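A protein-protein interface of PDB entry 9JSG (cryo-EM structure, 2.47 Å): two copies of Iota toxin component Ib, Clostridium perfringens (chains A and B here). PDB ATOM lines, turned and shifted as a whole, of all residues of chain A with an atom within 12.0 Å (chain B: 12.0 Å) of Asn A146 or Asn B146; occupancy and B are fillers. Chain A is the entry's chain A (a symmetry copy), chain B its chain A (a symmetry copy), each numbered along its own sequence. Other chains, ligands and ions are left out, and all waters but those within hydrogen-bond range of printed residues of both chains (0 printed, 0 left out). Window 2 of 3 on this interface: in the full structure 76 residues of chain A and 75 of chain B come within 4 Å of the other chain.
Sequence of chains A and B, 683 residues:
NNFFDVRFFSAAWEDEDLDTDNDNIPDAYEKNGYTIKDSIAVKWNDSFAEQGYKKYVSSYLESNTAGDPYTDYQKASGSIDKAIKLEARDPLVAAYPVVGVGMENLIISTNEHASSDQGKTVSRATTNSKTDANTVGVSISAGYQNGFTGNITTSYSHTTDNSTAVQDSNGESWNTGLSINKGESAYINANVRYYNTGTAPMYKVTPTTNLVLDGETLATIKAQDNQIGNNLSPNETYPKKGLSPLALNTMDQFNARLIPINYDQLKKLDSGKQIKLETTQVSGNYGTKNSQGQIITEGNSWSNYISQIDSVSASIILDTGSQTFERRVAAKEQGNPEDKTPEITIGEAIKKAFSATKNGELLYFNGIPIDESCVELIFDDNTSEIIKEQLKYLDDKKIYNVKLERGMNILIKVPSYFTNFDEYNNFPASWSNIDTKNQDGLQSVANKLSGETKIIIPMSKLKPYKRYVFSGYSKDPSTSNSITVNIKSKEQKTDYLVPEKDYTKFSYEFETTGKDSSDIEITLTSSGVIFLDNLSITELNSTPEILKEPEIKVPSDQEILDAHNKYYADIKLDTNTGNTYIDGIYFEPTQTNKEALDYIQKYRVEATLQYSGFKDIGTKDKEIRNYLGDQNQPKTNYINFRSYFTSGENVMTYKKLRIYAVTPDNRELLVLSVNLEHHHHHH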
ATOM      1  N   SER A 141       2.281 -33.034  11.675  1.00  0.00           N
ATOM      2  CA  SER A 141       1.576 -31.807  12.012  1.00  0.00           C
ATOM      3  C   SER A 141       0.209 -31.797  11.347  1.00  0.00           C
ATOM      4  O   SER A 141       0.065 -32.226  10.200  1.00  0.00           O
ATOM      5  CB  SER A 141       2.374 -30.570  11.579  1.00  0.00           C
ATOM      6  OG  SER A 141       1.582 -29.398  11.667  1.00  0.00           O
ATOM      7  N   ALA A 142      -0.794 -31.316  12.079  1.00  0.00           N
ATOM      8  CA  ALA A 142      -2.150 -31.180  11.563  1.00  0.00           C
ATOM      9  C   ALA A 142      -2.770 -29.917  12.137  1.00  0.00           C
ATOM     10  O   ALA A 142      -2.596 -29.625  13.324  1.00  0.00           O
ATOM     11  CB  ALA A 142      -3.008 -32.402  11.918  1.00  0.00           C
ATOM     12  N   GLY A 143      -3.487 -29.171  11.300  1.00  0.00           N
ATOM     13  CA  GLY A 143      -4.076 -27.930  11.759  1.00  0.00           C
ATOM     14  C   GLY A 143      -5.113 -27.395  10.795  1.00  0.00           C
ATOM     15  O   GLY A 143      -5.458 -28.033   9.796  1.00  0.00           O
ATOM     16  N   TYR A 144      -5.609 -26.204  11.117  1.00  0.00           N
ATOM     17  CA  TYR A 144      -6.610 -25.506  10.316  1.00  0.00           C
ATOM     18  C   TYR A 144      -6.110 -24.099  10.017  1.00  0.00           C
ATOM     19  O   TYR A 144      -6.134 -23.229  10.893  1.00  0.00           O
ATOM     20  CB  TYR A 144      -7.960 -25.463  11.034  1.00  0.00           C
ATOM     21  CG  TYR A 144      -9.044 -24.747  10.258  1.00  0.00           C
ATOM     22  CD1 TYR A 144      -9.790 -25.411   9.294  1.00  0.00           C
ATOM     23  CD2 TYR A 144      -9.326 -23.408  10.496  1.00  0.00           C
ATOM     24  CE1 TYR A 144     -10.781 -24.761   8.584  1.00  0.00           C
ATOM     25  CE2 TYR A 144     -10.315 -22.749   9.791  1.00  0.00           C
ATOM     26  CZ  TYR A 144     -11.039 -23.430   8.835  1.00  0.00           C
ATOM     27  N   GLN A 145      -5.656 -23.881   8.782  1.00  0.00           N
ATOM     28  CA  GLN A 145      -5.272 -22.557   8.296  1.00  0.00           C
ATOM     29  C   GLN A 145      -5.952 -22.344   6.941  1.00  0.00           C
ATOM     30  O   GLN A 145      -5.389 -22.656   5.891  1.00  0.00           O
ATOM     31  CB  GLN A 145      -3.753 -22.416   8.197  1.00  0.00           C
ATOM     32  CG  GLN A 145      -3.273 -20.981   8.054  1.00  0.00           C
ATOM     33  CD  GLN A 145      -1.764 -20.857   8.130  1.00  0.00           C
ATOM     34  OE1 GLN A 145      -1.144 -20.170   7.318  1.00  0.00           O
ATOM     35  NE2 GLN A 145      -1.166 -21.527   9.107  1.00  0.00           N
ATOM     36  N   ASN A 146      -7.174 -21.805   6.983  1.00  0.00           N
ATOM     37  CA  ASN A 146      -8.024 -21.674   5.804  1.00  0.00           C
ATOM     38  C   ASN A 146      -8.199 -23.027   5.124  1.00  0.00           C
ATOM     39  O   ASN A 146      -8.124 -23.131   3.895  1.00  0.00           O
ATOM     40  CB  ASN A 146      -7.448 -20.646   4.826  1.00  0.00           C
ATOM     41  CG  ASN A 146      -7.963 -19.243   5.086  1.00  0.00           C
ATOM     42  OD1 ASN A 146      -7.770 -18.689   6.166  1.00  0.00           O
ATOM     43  ND2 ASN A 146      -8.625 -18.662   4.091  1.00  0.00           N
ATOM     44  N   GLY A 147      -8.431 -24.063   5.918  1.00  0.00           N
ATOM     45  CA  GLY A 147      -8.566 -25.418   5.426  1.00  0.00           C
ATOM     46  C   GLY A 147      -7.883 -26.422   6.338  1.00  0.00           C
ATOM     47  O   GLY A 147      -7.076 -26.083   7.202  1.00  0.00           O
ATOM     48  N   PHE A 148      -8.234 -27.686   6.119  1.00  0.00           N
ATOM     49  CA  PHE A 148      -7.696 -28.794   6.903  1.00  0.00           C
ATOM     50  C   PHE A 148      -6.339 -29.177   6.324  1.00  0.00           C
ATOM     51  O   PHE A 148      -6.269 -29.859   5.298  1.00  0.00           O
ATOM     52  CB  PHE A 148      -8.650 -29.992   6.891  1.00  0.00           C
ATOM     53  CG  PHE A 148      -9.935 -29.776   7.655  1.00  0.00           C
ATOM     54  CD1 PHE A 148     -10.361 -28.506   8.013  1.00  0.00           C
ATOM     55  CD2 PHE A 148     -10.722 -30.860   8.009  1.00  0.00           C
ATOM     56  CE1 PHE A 148     -11.542 -28.323   8.709  1.00  0.00           C
ATOM     57  CE2 PHE A 148     -11.904 -30.684   8.706  1.00  0.00           C
ATOM     58  CZ  PHE A 148     -12.314 -29.413   9.056  1.00  0.00           C
ATOM     59  N   THR A 149      -5.264 -28.743   6.975  1.00  0.00           N
ATOM     60  CA  THR A 149      -3.918 -28.969   6.473  1.00  0.00           C
ATOM     61  C   THR A 149      -3.174 -29.987   7.331  1.00  0.00           C
ATOM     62  O   THR A 149      -3.378 -30.085   8.544  1.00  0.00           O
ATOM     63  CB  THR A 149      -3.127 -27.658   6.421  1.00  0.00           C
ATOM     64  OG1 THR A 149      -2.489 -27.432   7.683  1.00  0.00           O
ATOM     65  CG2 THR A 149      -4.046 -26.489   6.102  1.00  0.00           C
ATOM     66  N   GLY A 150      -2.298 -30.748   6.674  1.00  0.00           N
ATOM     67  CA  GLY A 150      -1.467 -31.724   7.347  1.00  0.00           C
ATOM     68  C   GLY A 150      -0.104 -31.786   6.692  1.00  0.00           C
ATOM     69  O   GLY A 150       0.088 -31.336   5.560  1.00  0.00           O
ATOM     70  N   ASN A 151       0.852 -32.355   7.425  1.00  0.00           N
ATOM     71  CA  ASN A 151       2.226 -32.408   6.946  1.00  0.00           C
ATOM     72  C   ASN A 151       2.969 -33.511   7.685  1.00  0.00           C
ATOM     73  O   ASN A 151       2.764 -33.710   8.885  1.00  0.00           O
ATOM     74  CB  ASN A 151       2.922 -31.049   7.137  1.00  0.00           C
ATOM     75  CG  ASN A 151       4.427 -31.103   6.898  1.00  0.00           C
ATOM     76  OD1 ASN A 151       5.169 -31.777   7.616  1.00  0.00           O
ATOM     77  ND2 ASN A 151       4.881 -30.389   5.876  1.00  0.00           N
ATOM     78  N   ALA B 142       6.279 -33.619   3.104  1.00  0.00           N
ATOM     79  CA  ALA B 142       5.158 -33.761   2.183  1.00  0.00           C
ATOM     80  C   ALA B 142       3.864 -33.530   2.945  1.00  0.00           C
ATOM     81  O   ALA B 142       3.717 -34.006   4.074  1.00  0.00           O
ATOM     82  CB  ALA B 142       5.148 -35.146   1.524  1.00  0.00           C
ATOM     83  N   GLY B 143       2.932 -32.805   2.332  1.00  0.00           N
ATOM     84  CA  GLY B 143       1.686 -32.505   3.008  1.00  0.00           C
ATOM     85  C   GLY B 143       0.634 -31.971   2.061  1.00  0.00           C
ATOM     86  O   GLY B 143       0.826 -31.912   0.844  1.00  0.00           O
ATOM     87  N   TYR B 144      -0.495 -31.581   2.648  1.00  0.00           N
ATOM     88  CA  TYR B 144      -1.630 -31.025   1.918  1.00  0.00           C
ATOM     89  C   TYR B 144      -2.023 -29.696   2.552  1.00  0.00           C
ATOM     90  O   TYR B 144      -2.638 -29.673   3.623  1.00  0.00           O
ATOM     91  CB  TYR B 144      -2.813 -31.995   1.913  1.00  0.00           C
ATOM     92  CG  TYR B 144      -4.029 -31.476   1.176  1.00  0.00           C
ATOM     93  CD1 TYR B 144      -4.145 -31.622  -0.198  1.00  0.00           C
ATOM     94  CD2 TYR B 144      -5.062 -30.848   1.858  1.00  0.00           C
ATOM     95  CE1 TYR B 144      -5.254 -31.150  -0.877  1.00  0.00           C
ATOM     96  CE2 TYR B 144      -6.175 -30.373   1.190  1.00  0.00           C
ATOM     97  CZ  TYR B 144      -6.265 -30.527  -0.178  1.00  0.00           C
ATOM     98  N   GLN B 145      -1.664 -28.594   1.892  1.00  0.00           N
ATOM     99  CA  GLN B 145      -2.083 -27.252   2.292  1.00  0.00           C
ATOM    100  C   GLN B 145      -2.621 -26.543   1.047  1.00  0.00           C
ATOM    101  O   GLN B 145      -1.882 -25.865   0.331  1.00  0.00           O
ATOM    102  CB  GLN B 145      -0.931 -26.476   2.935  1.00  0.00           C
ATOM    103  CG  GLN B 145      -1.371 -25.235   3.693  1.00  0.00           C
ATOM    104  CD  GLN B 145      -0.237 -24.584   4.459  1.00  0.00           C
ATOM    105  OE1 GLN B 145      -0.062 -23.367   4.415  1.00  0.00           O
ATOM    106  NE2 GLN B 145       0.541 -25.396   5.165  1.00  0.00           N
ATOM    107  N   ASN B 146      -3.924 -26.709   0.802  1.00  0.00           N
ATOM    108  CA  ASN B 146      -4.569 -26.233  -0.417  1.00  0.00           C
ATOM    109  C   ASN B 146      -3.851 -26.782  -1.643  1.00  0.00           C
ATOM    110  O   ASN B 146      -3.609 -26.053  -2.612  1.00  0.00           O
ATOM    111  CB  ASN B 146      -4.611 -24.703  -0.452  1.00  0.00           C
ATOM    112  CG  ASN B 146      -5.873 -24.141   0.177  1.00  0.00           C
ATOM    113  OD1 ASN B 146      -6.148 -24.367   1.354  1.00  0.00           O
ATOM    114  ND2 ASN B 146      -6.648 -23.403  -0.611  1.00  0.00           N
ATOM    115  N   GLY B 147      -3.510 -28.062  -1.608  1.00  0.00           N
ATOM    116  CA  GLY B 147      -2.777 -28.713  -2.673  1.00  0.00           C
ATOM    117  C   GLY B 147      -1.729 -29.671  -2.136  1.00  0.00           C
ATOM    118  O   GLY B 147      -1.362 -29.656  -0.962  1.00  0.00           O
ATOM    119  N   PHE B 148      -1.249 -30.520  -3.042  1.00  0.00           N
ATOM    120  CA  PHE B 148      -0.246 -31.528  -2.714  1.00  0.00           C
ATOM    121  C   PHE B 148       1.127 -30.867  -2.756  1.00  0.00           C
ATOM    122  O   PHE B 148       1.685 -30.652  -3.837  1.00  0.00           O
ATOM    123  CB  PHE B 148      -0.311 -32.707  -3.688  1.00  0.00           C
ATOM    124  CG  PHE B 148      -1.546 -33.566  -3.550  1.00  0.00           C
ATOM    125  CD1 PHE B 148      -2.667 -33.117  -2.869  1.00  0.00           C
ATOM    126  CD2 PHE B 148      -1.580 -34.830  -4.115  1.00  0.00           C
ATOM    127  CE1 PHE B 148      -3.793 -33.912  -2.754  1.00  0.00           C
ATOM    128  CE2 PHE B 148      -2.703 -35.630  -4.003  1.00  0.00           C
ATOM    129  CZ  PHE B 148      -3.811 -35.169  -3.320  1.00  0.00           C
ATOM    130  N   THR B 149       1.675 -30.545  -1.588  1.00  0.00           N
ATOM    131  CA  THR B 149       2.940 -29.832  -1.502  1.00  0.00           C
ATOM    132  C   THR B 149       4.050 -30.743  -0.987  1.00  0.00           C
ATOM    133  O   THR B 149       3.825 -31.649  -0.181  1.00  0.00           O
ATOM    134  CB  THR B 149       2.814 -28.604  -0.595  1.00  0.00           C
ATOM    135  OG1 THR B 149       3.072 -28.981   0.762  1.00  0.00           O
ATOM    136  CG2 THR B 149       1.421 -28.002  -0.698  1.00  0.00           C
ATOM    137  N   GLY B 150       5.266 -30.482  -1.471  1.00  0.00           N
ATOM    138  CA  GLY B 150       6.440 -31.214  -1.043  1.00  0.00           C
ATOM    139  C   GLY B 150       7.637 -30.290  -0.991  1.00  0.00           C
ATOM    140  O   GLY B 150       7.639 -29.205  -1.578  1.00  0.00           O
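O of Gly A150 is in hydrogen-bond range of N of Tyr B144 (3.0 Å).
The side-chain amide oxygen (OD1) of Asn B146 lies close to the backbone carbonyl oxygen (O) of Asn A146.
N of Gly B143 lies within hydrogen-bond range of O of Thr B149.
O of Ser A141 sits at hydrogen-bond distance from N of Asn A151 (2.9 Å).
The backbone carbonyl oxygen (O) of Thr A149 is in hydrogen-bond range of the backbone NH (N) of Gly A143 (2.9 Å).
O of Phe A148 touches CD2 of Tyr B144, at 3.8 Å.
Thr A149 touches Tyr B144 (CA to O, 3.2 Å).
Thr A149 touches Gln B145 (CG2 to CG, 3.8 Å).
Gly B143 touches Gly A150 (CA to O, 3.2 Å).
Asn A151 touches Ala B142.
CA of Asn A151 touches CA of Gly B143, 3.98 Å away.
Of the printed residues of chain B, Asn A146 touches Asn B146 (3.4 Å).
Of chain A, only Asn A146 comes within 4 Å of Asn B146.
No residue of chain B comes within 4 Å of Tyr A144.
No residue of chain B comes within 4 Å of Gln A145.
No residue of chain B comes within 4 Å of Gly A147.
Tyr B144 touches three residues of chain A.
No residue of chain A comes within 4 Å of Gly B147.
Of the printed residues of chain B, Asn A151 touches Ala B142 (3.6 Å) and Gly B143 (3.98 Å).
Of the printed residues of chain B, Phe A148 touches Tyr B144.
Of the printed residues of chain B, Thr A149 touches Tyr B144 (3.2 Å) and Gln B145 (3.8 Å).
Printed residues of chain A within 4 Å of Gly B143: Gly A150 (3.2 Å) and Asn A151 (3.98 Å).
Of the printed residues of chain A, Ala B142 touches Asn A151 (3.6 Å).
Phe B148 touches none of the printed residues of chain A.
Gly B150 touches none of the printed residues of chain A.
The nearest residue of chain A that does not touch Asn B146 is Gly A147 (4.9 Å).
The nearest printed residue of chain B that does not touch Phe A148 is Gln B145 (5.8 Å).
Along chain A the printed residues that touch a printed residue of chain B span positions 146 to 151.
Of the 9 printed residues of chain B, 5 touch a printed residue of chain A.
Among the printed residues, no Asp or Glu carboxylate lies within 4 Å of a Lys or Arg side-chain nitrogen of the other chain.
Phe A148 touches Tyr B144, but with the chains exchanged Tyr A144 does not touch Phe B148 (15.2 Å).
Thr A149 touches Gln B145, but with the chains exchanged Gln A145 does not touch Thr B149 (10.9 Å).
Gly A150 touches Gly B143, but with the chains exchanged Gly A143 does not touch Gly B150 (15.5 Å).
Gly A150 touches Tyr B144, but with the chains exchanged Tyr A144 does not touch Gly B150 (17.2 Å).
Of the 8 pairs that touch across the chains among the printed residues, 1 has its exchanged pair printed and touching as well.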
